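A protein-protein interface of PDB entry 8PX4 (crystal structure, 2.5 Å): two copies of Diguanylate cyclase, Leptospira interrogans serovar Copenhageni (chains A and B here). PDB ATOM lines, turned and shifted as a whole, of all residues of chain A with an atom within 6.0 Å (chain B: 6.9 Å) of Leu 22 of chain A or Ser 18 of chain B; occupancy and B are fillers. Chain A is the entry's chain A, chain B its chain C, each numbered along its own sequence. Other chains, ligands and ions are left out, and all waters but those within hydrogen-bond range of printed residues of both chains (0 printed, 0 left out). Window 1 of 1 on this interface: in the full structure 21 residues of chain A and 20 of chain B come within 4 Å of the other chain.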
ATOM      1  N   LEU A  14     -15.679 -34.136  -5.487  1.00  0.00           N
ATOM      2  CA  LEU A  14     -15.739 -32.782  -4.980  1.00  0.00           C
ATOM      3  C   LEU A  14     -17.056 -32.139  -5.401  1.00  0.00           C
ATOM      4  O   LEU A  14     -17.764 -31.559  -4.572  1.00  0.00           O
ATOM      5  CB  LEU A  14     -14.526 -32.027  -5.522  1.00  0.00           C
ATOM      6  CG  LEU A  14     -14.304 -30.622  -4.998  1.00  0.00           C
ATOM      7  CD1 LEU A  14     -14.249 -30.599  -3.480  1.00  0.00           C
ATOM      8  CD2 LEU A  14     -13.002 -30.042  -5.586  1.00  0.00           C
ATOM      9  N   VAL A  15     -17.414 -32.305  -6.676  1.00  0.00           N
ATOM     10  CA  VAL A  15     -18.626 -31.693  -7.195  1.00  0.00           C
ATOM     11  C   VAL A  15     -19.852 -32.381  -6.583  1.00  0.00           C
ATOM     12  O   VAL A  15     -20.833 -31.710  -6.242  1.00  0.00           O
ATOM     13  CB  VAL A  15     -18.677 -31.688  -8.735  1.00  0.00           C
ATOM     14  CG1 VAL A  15     -17.618 -30.763  -9.314  1.00  0.00           C
ATOM     15  CG2 VAL A  15     -18.579 -33.081  -9.341  1.00  0.00           C
ATOM     16  N   ASN A  16     -19.775 -33.700  -6.403  1.00  0.00           N
ATOM     17  CA  ASN A  16     -20.944 -34.477  -6.026  1.00  0.00           C
ATOM     18  C   ASN A  16     -21.215 -34.362  -4.521  1.00  0.00           C
ATOM     19  O   ASN A  16     -22.292 -34.756  -4.066  1.00  0.00           O
ATOM     20  CB  ASN A  16     -20.803 -35.943  -6.429  1.00  0.00           C
ATOM     21  CG  ASN A  16     -20.986 -36.172  -7.914  1.00  0.00           C
ATOM     22  OD1 ASN A  16     -21.596 -35.363  -8.615  1.00  0.00           O
ATOM     23  ND2 ASN A  16     -20.466 -37.280  -8.399  1.00  0.00           N
ATOM     24  N   SER A  18     -21.021 -31.374  -2.911  1.00  0.00           N
ATOM     25  CA  SER A  18     -21.463 -30.011  -2.640  1.00  0.00           C
ATOM     26  C   SER A  18     -22.969 -29.982  -2.348  1.00  0.00           C
ATOM     27  O   SER A  18     -23.754 -30.625  -3.035  1.00  0.00           O
ATOM     28  CB  SER A  18     -21.129 -29.113  -3.774  1.00  0.00           C
ATOM     29  OG  SER A  18     -21.508 -27.775  -3.490  1.00  0.00           O
ATOM     30  N   ASP A  20     -24.555 -27.302  -2.727  1.00  0.00           N
ATOM     31  CA  ASP A  20     -25.032 -26.340  -3.707  1.00  0.00           C
ATOM     32  C   ASP A  20     -25.153 -27.022  -5.068  1.00  0.00           C
ATOM     33  O   ASP A  20     -24.515 -28.038  -5.325  1.00  0.00           O
ATOM     34  CB  ASP A  20     -24.132 -25.111  -3.723  1.00  0.00           C
ATOM     35  CG  ASP A  20     -24.405 -24.154  -2.565  1.00  0.00           C
ATOM     36  OD1 ASP A  20     -25.398 -24.364  -1.830  1.00  0.00           O
ATOM     37  OD2 ASP A  20     -23.681 -23.161  -2.461  1.00  0.00           O
ATOM     38  N   LEU A  21     -26.044 -26.481  -5.906  1.00  0.00           N
ATOM     39  CA  LEU A  21     -26.273 -27.004  -7.241  1.00  0.00           C
ATOM     40  C   LEU A  21     -25.069 -26.663  -8.128  1.00  0.00           C
ATOM     41  O   LEU A  21     -24.694 -25.503  -8.259  1.00  0.00           O
ATOM     42  CB  LEU A  21     -27.559 -26.392  -7.801  1.00  0.00           C
ATOM     43  CG  LEU A  21     -28.811 -26.537  -6.923  1.00  0.00           C
ATOM     44  CD1 LEU A  21     -29.734 -25.350  -7.112  1.00  0.00           C
ATOM     45  CD2 LEU A  21     -29.552 -27.823  -7.219  1.00  0.00           C
ATOM     46  N   LEU A  22     -24.450 -27.696  -8.699  1.00  0.00           N
ATOM     47  CA  LEU A  22     -23.390 -27.525  -9.674  1.00  0.00           C
ATOM     48  C   LEU A  22     -23.803 -28.209 -10.969  1.00  0.00           C
ATOM     49  O   LEU A  22     -24.102 -29.405 -10.971  1.00  0.00           O
ATOM     50  CB  LEU A  22     -22.101 -28.136  -9.127  1.00  0.00           C
ATOM     51  CG  LEU A  22     -21.470 -27.422  -7.936  1.00  0.00           C
ATOM     52  CD1 LEU A  22     -20.317 -28.242  -7.377  1.00  0.00           C
ATOM     53  CD2 LEU A  22     -20.987 -26.045  -8.323  1.00  0.00           C
ATOM     54  N   SER A  23     -23.806 -27.444 -12.060  1.00  0.00           N
ATOM     55  CA  SER A  23     -24.272 -27.948 -13.332  1.00  0.00           C
ATOM     56  C   SER A  23     -23.416 -27.412 -14.481  1.00  0.00           C
ATOM     57  O   SER A  23     -22.861 -26.323 -14.402  1.00  0.00           O
ATOM     58  CB  SER A  23     -25.720 -27.623 -13.535  1.00  0.00           C
ATOM     59  OG  SER A  23     -26.198 -28.225 -14.729  1.00  0.00           O
ATOM     60  N   ILE A  24     -23.315 -28.219 -15.539  1.00  0.00           N
ATOM     61  CA  ILE A  24     -22.767 -27.790 -16.810  1.00  0.00           C
ATOM     62  C   ILE A  24     -23.883 -27.869 -17.850  1.00  0.00           C
ATOM     63  O   ILE A  24     -24.564 -28.896 -17.959  1.00  0.00           O
ATOM     64  CB  ILE A  24     -21.543 -28.657 -17.199  1.00  0.00           C
ATOM     65  CG1 ILE A  24     -20.452 -28.599 -16.128  1.00  0.00           C
ATOM     66  CG2 ILE A  24     -21.005 -28.275 -18.572  1.00  0.00           C
ATOM     67  CD1 ILE A  24     -19.389 -29.654 -16.282  1.00  0.00           C
ATOM     68  N   GLN A  33     -24.571 -32.026 -17.193  1.00  0.00           N
ATOM     69  CA  GLN A  33     -24.158 -32.558 -15.904  1.00  0.00           C
ATOM     70  C   GLN A  33     -24.940 -31.867 -14.784  1.00  0.00           C
ATOM     71  O   GLN A  33     -25.242 -30.675 -14.857  1.00  0.00           O
ATOM     72  CB  GLN A  33     -22.643 -32.385 -15.727  1.00  0.00           C
ATOM     73  CG  GLN A  33     -22.074 -33.078 -14.492  1.00  0.00           C
ATOM     74  CD  GLN A  33     -22.184 -32.247 -13.229  1.00  0.00           C
ATOM     75  OE1 GLN A  33     -22.345 -31.026 -13.264  1.00  0.00           O
ATOM     76  NE2 GLN A  33     -22.104 -32.917 -12.090  1.00  0.00           N
ATOM     77  N   VAL A  34     -25.265 -32.646 -13.757  1.00  0.00           N
ATOM     78  CA  VAL A  34     -25.848 -32.133 -12.536  1.00  0.00           C
ATOM     79  C   VAL A  34     -25.304 -32.972 -11.384  1.00  0.00           C
ATOM     80  O   VAL A  34     -24.993 -34.146 -11.564  1.00  0.00           O
ATOM     81  CB  VAL A  34     -27.395 -32.161 -12.565  1.00  0.00           C
ATOM     82  CG1 VAL A  34     -27.984 -31.040 -13.417  1.00  0.00           C
ATOM     83  CG2 VAL A  34     -27.933 -33.513 -13.007  1.00  0.00           C
ATOM     84  N   ASN A  35     -25.196 -32.358 -10.208  1.00  0.00           N
ATOM     85  CA  ASN A  35     -24.717 -33.048  -9.030  1.00  0.00           C
ATOM     86  C   ASN A  35     -25.925 -33.480  -8.200  1.00  0.00           C
ATOM     87  O   ASN A  35     -27.043 -33.047  -8.472  1.00  0.00           O
ATOM     88  CB  ASN A  35     -23.719 -32.186  -8.253  1.00  0.00           C
ATOM     89  CG  ASN A  35     -24.328 -30.951  -7.622  1.00  0.00           C
ATOM     90  OD1 ASN A  35     -25.400 -30.508  -8.011  1.00  0.00           O
ATOM     91  ND2 ASN A  35     -23.626 -30.362  -6.675  1.00  0.00           N
ATOM     92  N   ALA A  37     -27.197 -32.664  -5.606  1.00  0.00           N
ATOM     93  CA  ALA A  37     -27.885 -31.579  -4.928  1.00  0.00           C
ATOM     94  C   ALA A  37     -29.210 -31.264  -5.633  1.00  0.00           C
ATOM     95  O   ALA A  37     -30.152 -30.802  -5.003  1.00  0.00           O
ATOM     96  CB  ALA A  37     -26.982 -30.370  -4.882  1.00  0.00           C
ATOM     97  N   PHE A  38     -29.252 -31.476  -6.956  1.00  0.00           N
ATOM     98  CA  PHE A  38     -30.458 -31.219  -7.730  1.00  0.00           C
ATOM     99  C   PHE A  38     -31.576 -32.160  -7.275  1.00  0.00           C
ATOM    100  O   PHE A  38     -32.699 -31.725  -7.070  1.00  0.00           O
ATOM    101  CB  PHE A  38     -30.187 -31.369  -9.227  1.00  0.00           C
ATOM    102  CG  PHE A  38     -29.645 -30.134  -9.902  1.00  0.00           C
ATOM    103  CD1 PHE A  38     -28.281 -29.862  -9.913  1.00  0.00           C
ATOM    104  CD2 PHE A  38     -30.501 -29.229 -10.514  1.00  0.00           C
ATOM    105  CE1 PHE A  38     -27.788 -28.730 -10.545  1.00  0.00           C
ATOM    106  CE2 PHE A  38     -30.004 -28.102 -11.150  1.00  0.00           C
ATOM    107  CZ  PHE A  38     -28.652 -27.857 -11.171  1.00  0.00           C
ATOM    108  N   VAL A 111     -22.428 -23.560 -13.989  1.00  0.00           N
ATOM    109  CA  VAL A 111     -23.526 -23.031 -13.193  1.00  0.00           C
ATOM    110  C   VAL A 111     -23.296 -23.408 -11.732  1.00  0.00           C
ATOM    111  O   VAL A 111     -23.009 -24.571 -11.422  1.00  0.00           O
ATOM    112  CB  VAL A 111     -24.895 -23.542 -13.689  1.00  0.00           C
ATOM    113  CG1 VAL A 111     -26.035 -22.817 -13.000  1.00  0.00           C
ATOM    114  CG2 VAL A 111     -25.037 -23.430 -15.200  1.00  0.00           C
ATOM    115  N   THR A 112     -23.476 -22.415 -10.848  1.00  0.00           N
ATOM    116  CA  THR A 112     -23.579 -22.654  -9.422  1.00  0.00           C
ATOM    117  C   THR A 112     -24.904 -22.093  -8.927  1.00  0.00           C
ATOM    118  O   THR A 112     -25.295 -20.988  -9.299  1.00  0.00           O
ATOM    119  CB  THR A 112     -22.411 -22.014  -8.667  1.00  0.00           C
ATOM    120  OG1 THR A 112     -21.176 -22.543  -9.157  1.00  0.00           O
ATOM    121  CG2 THR A 112     -22.486 -22.249  -7.175  1.00  0.00           C
ATOM    122  N   GLY A 113     -25.592 -22.873  -8.092  1.00  0.00           N
ATOM    123  CA  GLY A 113     -26.919 -22.525  -7.626  1.00  0.00           C
ATOM    124  C   GLY A 113     -27.059 -22.720  -6.125  1.00  0.00           C
ATOM    125  O   GLY A 113     -26.479 -23.633  -5.555  1.00  0.00           O
ATOM    126  N   LYS B  13     -12.932 -27.051 -15.017  1.00  0.00           N
ATOM    127  CA  LYS B  13     -13.432 -25.727 -15.347  1.00  0.00           C
ATOM    128  C   LYS B  13     -14.677 -25.427 -14.508  1.00  0.00           C
ATOM    129  O   LYS B  13     -14.964 -24.280 -14.213  1.00  0.00           O
ATOM    130  CB  LYS B  13     -13.727 -25.642 -16.849  1.00  0.00           C
ATOM    131  CG  LYS B  13     -12.510 -25.767 -17.757  1.00  0.00           C
ATOM    132  CD  LYS B  13     -12.097 -24.456 -18.392  1.00  0.00           C
ATOM    133  CE  LYS B  13     -10.875 -24.581 -19.279  1.00  0.00           C
ATOM    134  NZ  LYS B  13     -10.373 -23.253 -19.712  1.00  0.00           N
ATOM    135  N   LEU B  14     -15.405 -26.476 -14.123  1.00  0.00           N
ATOM    136  CA  LEU B  14     -16.581 -26.329 -13.283  1.00  0.00           C
ATOM    137  C   LEU B  14     -16.144 -25.969 -11.862  1.00  0.00           C
ATOM    138  O   LEU B  14     -16.679 -25.048 -11.257  1.00  0.00           O
ATOM    139  CB  LEU B  14     -17.384 -27.641 -13.320  1.00  0.00           C
ATOM    140  CG  LEU B  14     -18.647 -27.684 -12.447  1.00  0.00           C
ATOM    141  CD1 LEU B  14     -19.656 -26.633 -12.890  1.00  0.00           C
ATOM    142  CD2 LEU B  14     -19.278 -29.073 -12.472  1.00  0.00           C
ATOM    143  N   VAL B  15     -15.140 -26.680 -11.358  1.00  0.00           N
ATOM    144  CA  VAL B  15     -14.619 -26.459 -10.020  1.00  0.00           C
ATOM    145  C   VAL B  15     -14.032 -25.047  -9.915  1.00  0.00           C
ATOM    146  O   VAL B  15     -14.260 -24.349  -8.933  1.00  0.00           O
ATOM    147  CB  VAL B  15     -13.585 -27.549  -9.668  1.00  0.00           C
ATOM    148  CG1 VAL B  15     -12.687 -27.157  -8.501  1.00  0.00           C
ATOM    149  CG2 VAL B  15     -14.276 -28.883  -9.405  1.00  0.00           C
ATOM    150  N   ASN B  16     -13.297 -24.625 -10.939  1.00  0.00           N
ATOM    151  CA  ASN B  16     -12.504 -23.407 -10.842  1.00  0.00           C
ATOM    152  C   ASN B  16     -13.365 -22.175 -11.139  1.00  0.00           C
ATOM    153  O   ASN B  16     -12.940 -21.067 -10.881  1.00  0.00           O
ATOM    154  CB  ASN B  16     -11.263 -23.457 -11.744  1.00  0.00           C
ATOM    155  CG  ASN B  16     -10.194 -24.393 -11.214  1.00  0.00           C
ATOM    156  OD1 ASN B  16     -10.063 -24.563 -10.001  1.00  0.00           O
ATOM    157  ND2 ASN B  16      -9.454 -25.037 -12.105  1.00  0.00           N
ATOM    158  N   ASN B  17     -14.580 -22.375 -11.657  1.00  0.00           N
ATOM    159  CA  ASN B  17     -15.474 -21.254 -11.953  1.00  0.00           C
ATOM    160  C   ASN B  17     -16.658 -21.245 -10.978  1.00  0.00           C
ATOM    161  O   ASN B  17     -17.617 -20.512 -11.181  1.00  0.00           O
ATOM    162  CB  ASN B  17     -15.973 -21.292 -13.401  1.00  0.00           C
ATOM    163  CG  ASN B  17     -14.942 -20.808 -14.395  1.00  0.00           C
ATOM    164  OD1 ASN B  17     -14.652 -19.617 -14.465  1.00  0.00           O
ATOM    165  ND2 ASN B  17     -14.379 -21.722 -15.161  1.00  0.00           N
ATOM    166  N   SER B  18     -16.569 -22.049  -9.915  1.00  0.00           N
ATOM    167  CA  SER B  18     -17.673 -22.216  -8.985  1.00  0.00           C
ATOM    168  C   SER B  18     -17.607 -21.161  -7.879  1.00  0.00           C
ATOM    169  O   SER B  18     -16.535 -20.828  -7.383  1.00  0.00           O
ATOM    170  CB  SER B  18     -17.687 -23.604  -8.413  1.00  0.00           C
ATOM    171  OG  SER B  18     -18.741 -23.746  -7.476  1.00  0.00           O
ATOM    172  N   LEU B  19     -18.789 -20.701  -7.458  1.00  0.00           N
ATOM    173  CA  LEU B  19     -18.925 -19.757  -6.362  1.00  0.00           C
ATOM    174  C   LEU B  19     -18.579 -20.452  -5.040  1.00  0.00           C
ATOM    175  O   LEU B  19     -18.230 -19.793  -4.071  1.00  0.00           O
ATOM    176  CB  LEU B  19     -20.370 -19.234  -6.364  1.00  0.00           C
ATOM    177  CG  LEU B  19     -20.596 -17.835  -5.794  1.00  0.00           C
ATOM    178  CD1 LEU B  19     -20.006 -16.768  -6.708  1.00  0.00           C
ATOM    179  CD2 LEU B  19     -22.088 -17.582  -5.568  1.00  0.00           C
ATOM    180  N   ASP B  20     -18.664 -21.784  -5.017  1.00  0.00           N
ATOM    181  CA  ASP B  20     -18.437 -22.531  -3.798  1.00  0.00           C
ATOM    182  C   ASP B  20     -16.944 -22.784  -3.609  1.00  0.00           C
ATOM    183  O   ASP B  20     -16.206 -22.924  -4.576  1.00  0.00           O
ATOM    184  CB  ASP B  20     -19.227 -23.842  -3.788  1.00  0.00           C
ATOM    185  CG  ASP B  20     -20.727 -23.629  -3.803  1.00  0.00           C
ATOM    186  OD1 ASP B  20     -21.172 -22.613  -3.234  1.00  0.00           O
ATOM    187  OD2 ASP B  20     -21.431 -24.448  -4.431  1.00  0.00           O
ATOM    188  N   LEU B  21     -16.529 -22.870  -2.341  1.00  0.00           N
ATOM    189  CA  LEU B  21     -15.196 -23.302  -1.983  1.00  0.00           C
ATOM    190  C   LEU B  21     -15.088 -24.802  -2.221  1.00  0.00           C
ATOM    191  O   LEU B  21     -15.885 -25.576  -1.690  1.00  0.00           O
ATOM    192  CB  LEU B  21     -14.945 -22.968  -0.511  1.00  0.00           C
ATOM    193  CG  LEU B  21     -15.134 -21.504  -0.124  1.00  0.00           C
ATOM    194  CD1 LEU B  21     -15.650 -21.383   1.303  1.00  0.00           C
ATOM    195  CD2 LEU B  21     -13.837 -20.741  -0.275  1.00  0.00           C
ATOM    196  N   LEU B  22     -14.109 -25.200  -3.038  1.00  0.00           N
ATOM    197  CA  LEU B  22     -13.856 -26.608  -3.294  1.00  0.00           C
ATOM    198  C   LEU B  22     -12.382 -26.894  -3.039  1.00  0.00           C
ATOM    199  O   LEU B  22     -11.508 -26.226  -3.583  1.00  0.00           O
ATOM    200  CB  LEU B  22     -14.267 -26.935  -4.737  1.00  0.00           C
ATOM    201  CG  LEU B  22     -15.751 -26.717  -5.062  1.00  0.00           C
ATOM    202  CD1 LEU B  22     -16.025 -26.875  -6.541  1.00  0.00           C
ATOM    203  CD2 LEU B  22     -16.641 -27.655  -4.260  1.00  0.00           C
ATOM    204  N   ASN B  35      -9.689 -23.977  -4.982  1.00  0.00           N
ATOM    205  CA  ASN B  35     -10.185 -23.333  -6.186  1.00  0.00           C
ATOM    206  C   ASN B  35     -10.164 -21.828  -5.959  1.00  0.00           C
ATOM    207  O   ASN B  35      -9.988 -21.375  -4.824  1.00  0.00           O
ATOM    208  CB  ASN B  35     -11.573 -23.856  -6.587  1.00  0.00           C
ATOM    209  CG  ASN B  35     -12.688 -23.464  -5.629  1.00  0.00           C
ATOM    210  OD1 ASN B  35     -12.446 -23.120  -4.475  1.00  0.00           O
ATOM    211  ND2 ASN B  35     -13.917 -23.549  -6.089  1.00  0.00           N
ATOM    212  N   PRO B  36     -10.298 -21.004  -7.030  1.00  0.00           N
ATOM    213  CA  PRO B  36     -10.140 -19.549  -6.901  1.00  0.00           C
ATOM    214  C   PRO B  36     -11.126 -18.896  -5.932  1.00  0.00           C
ATOM    215  O   PRO B  36     -10.927 -17.760  -5.522  1.00  0.00           O
ATOM    216  CB  PRO B  36     -10.366 -19.037  -8.337  1.00  0.00           C
ATOM    217  CG  PRO B  36      -9.994 -20.226  -9.214  1.00  0.00           C
ATOM    218  CD  PRO B  36     -10.472 -21.439  -8.439  1.00  0.00           C
ATOM    219  N   ALA B  37     -12.185 -19.623  -5.578  1.00  0.00           N
ATOM    220  CA  ALA B  37     -13.213 -19.122  -4.670  1.00  0.00           C
ATOM    221  C   ALA B  37     -12.620 -18.800  -3.294  1.00  0.00           C
ATOM    222  O   ALA B  37     -13.142 -17.945  -2.579  1.00  0.00           O
ATOM    223  CB  ALA B  37     -14.321 -20.137  -4.541  1.00  0.00           C
ATOM    224  N   PHE B  38     -11.562 -19.518  -2.904  1.00  0.00           N
ATOM    225  CA  PHE B  38     -10.910 -19.265  -1.624  1.00  0.00           C
ATOM    226  C   PHE B  38     -10.313 -17.861  -1.615  1.00  0.00           C
ATOM    227  O   PHE B  38     -10.480 -17.130  -0.643  1.00  0.00           O
ATOM    228  CB  PHE B  38      -9.849 -20.321  -1.319  1.00  0.00           C
ATOM    229  CG  PHE B  38     -10.383 -21.551  -0.635  1.00  0.00           C
ATOM    230  CD1 PHE B  38     -10.900 -22.604  -1.374  1.00  0.00           C
ATOM    231  CD2 PHE B  38     -10.387 -21.651   0.750  1.00  0.00           C
ATOM    232  CE1 PHE B  38     -11.397 -23.730  -0.740  1.00  0.00           C
ATOM    233  CE2 PHE B  38     -10.894 -22.777   1.382  1.00  0.00           C
ATOM    234  CZ  PHE B  38     -11.382 -23.819   0.637  1.00  0.00           C
ATOM    235  N   ARG B  40     -11.299 -15.406  -3.414  1.00  0.00           N
ATOM    236  CA  ARG B  40     -12.386 -14.449  -3.566  1.00  0.00           C
ATOM    237  C   ARG B  40     -13.070 -14.212  -2.213  1.00  0.00           C
ATOM    238  O   ARG B  40     -13.422 -13.084  -1.886  1.00  0.00           O
ATOM    239  CB  ARG B  40     -13.371 -14.964  -4.621  1.00  0.00           C
ATOM    240  CG  ARG B  40     -14.446 -13.964  -5.029  1.00  0.00           C
ATOM    241  CD  ARG B  40     -15.274 -14.436  -6.218  1.00  0.00           C
ATOM    242  NE  ARG B  40     -15.836 -15.770  -6.029  1.00  0.00           N
ATOM    243  CZ  ARG B  40     -16.859 -16.063  -5.227  1.00  0.00           C
ATOM    244  NH1 ARG B  40     -17.541 -15.100  -4.628  1.00  0.00           N
ATOM    245  NH2 ARG B  40     -17.198 -17.322  -5.035  1.00  0.00           N
ATOM    246  N   THR B 112     -16.302 -29.034   0.617  1.00  0.00           N
ATOM    247  CA  THR B 112     -17.115 -28.084  -0.118  1.00  0.00           C
ATOM    248  C   THR B 112     -17.660 -27.065   0.867  1.00  0.00           C
ATOM    249  O   THR B 112     -18.086 -27.426   1.956  1.00  0.00           O
ATOM    250  CB  THR B 112     -18.260 -28.769  -0.876  1.00  0.00           C
ATOM    251  OG1 THR B 112     -19.200 -29.218   0.091  1.00  0.00           O
ATOM    252  CG2 THR B 112     -17.794 -29.927  -1.733  1.00  0.00           C
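OD2 of Asp 20 of chain A lies close to OD1 of Asp 20 of chain B (2.7 Å).
OG of Ser 18 of chain A lies within hydrogen-bond range of OD2 of Asp 20 of chain B, at 3.5 Å.
N of Leu 19 of chain B lies within hydrogen-bond range of OG1 of Thr 112 of chain A (3.5 Å).
The side-chain hydroxyl (OG) of Ser 18 of chain B is in hydrogen-bond range of the side-chain hydroxyl (OG1) of Thr 112 of chain A (3.2 Å).
The side-chain amide nitrogen (ND2) of Asn 35 of chain B lies within hydrogen-bond range of the backbone carbonyl oxygen (O) of Asp 20 of chain B (2.8 Å).
OE1 of Gln 33 of chain A sits close to O of Leu 22 of chain A.
The backbone carbonyl oxygen of Val 15 of chain A lies within hydrogen-bond range of the side-chain amide nitrogen of Asn 35 of chain A, 3.1 Å away.
The backbone carbonyl oxygen (O) of Asp 20 of chain A lies within hydrogen-bond range of the side-chain amide nitrogen (ND2) of Asn 35 of chain A (2.8 Å).
The backbone NH (N) of Leu 22 of chain A sits at hydrogen-bond distance from the side-chain amide oxygen (OD1) of Asn 35 of chain A.
O of Ser 23 of chain A is in hydrogen-bond range of N of Val 111 of chain A (2.8 Å).
CB of Leu 22 of chain B touches CD2 of Leu 14 of chain A, at 3.5 Å.
Thr 112 of chain B touches Leu 14 of chain A (CG2 to O, 3.3 Å).
CD2 of Leu 14 of chain B touches CG1 of Val 15 of chain A (3.9 Å).
Val 15 of chain B touches Val 15 of chain A.
CA of Ser 18 of chain A touches OG1 of Thr 112 of chain B, 3.6 Å away.
Ser 18 of chain B touches Leu 22 of chain A (OG to CD2, 3.3 Å).
Ser 23 of chain A touches Leu 14 of chain B.
Leu 14 of chain B touches Ile 24 of chain A (CD2 to CD1, 3.9 Å).
OE1 of Gln 33 of chain A touches CD2 of Leu 14 of chain B, 3.7 Å away.
Thr 112 of chain A touches Asp 20 of chain B (CG2 to OD2, 3.7 Å).
Of the printed residues of chain B, Leu 22 of chain A touches Ser 18.
Ser 18 of chain B touches just these residues of chain A: Leu 22 (3.3 Å) and Thr 112 (3.2 Å).
Printed residues of chain B within 4 Å of Thr 112 of chain A: Ser 18 (3.2 Å), Leu 19 (3.5 Å) and Asp 20 (3.7 Å).
Printed residues of chain A within 4 Å of Leu 14 of chain B: Val 15 (3.9 Å), Ser 23 (3.6 Å), Ile 24 (3.9 Å) and Gln 33 (3.7 Å).
Of the printed residues of chain B, Val 15 of chain A touches Leu 14 and Val 15.
Printed residues of chain A within 4 Å of Val 15 of chain B: Val 15 (3.8 Å).
Phe 38 of chain B touches none of the printed residues of chain A.
The nearest residue of chain A that does not touch Ser 18 of chain B is Val 111 of chain A (5.9 Å).
The nearest printed residue of chain A that does not touch Asp 20 of chain B is Leu 22 of chain A (4.2 Å).
Of the 16 printed residues of chain B, 7 touch a printed residue of chain A.
Of the 17 printed residues of chain A, 9 touch a printed residue of chain B.
Printed residues of chain A that touch a printed residue of chain B: Leu 14, Val 15, Ser 18, Asp 20, Leu 22, Ser 23, Ile 24, Gln 33 and Thr 112.
Among the printed residues, no Asp or Glu carboxylate lies within 4 Å of a Lys or Arg side-chain nitrogen of the other chain.
Leu 14 of chain A touches Leu 22 of chain B, but with the chains exchanged Leu 22 of chain A does not touch Leu 14 of chain B (4.5 Å).
Val 15 of chain A touches Leu 14 of chain B, but with the chains exchanged Leu 14 of chain A does not touch Val 15 of chain B (4.1 Å).
Val 15 of chain A touches its own counterpart, Val 15 of chain B.
Ser 18 of chain A touches Asp 20 of chain B, but with the chains exchanged Asp 20 of chain A does not touch Ser 18 of chain B (6.7 Å).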
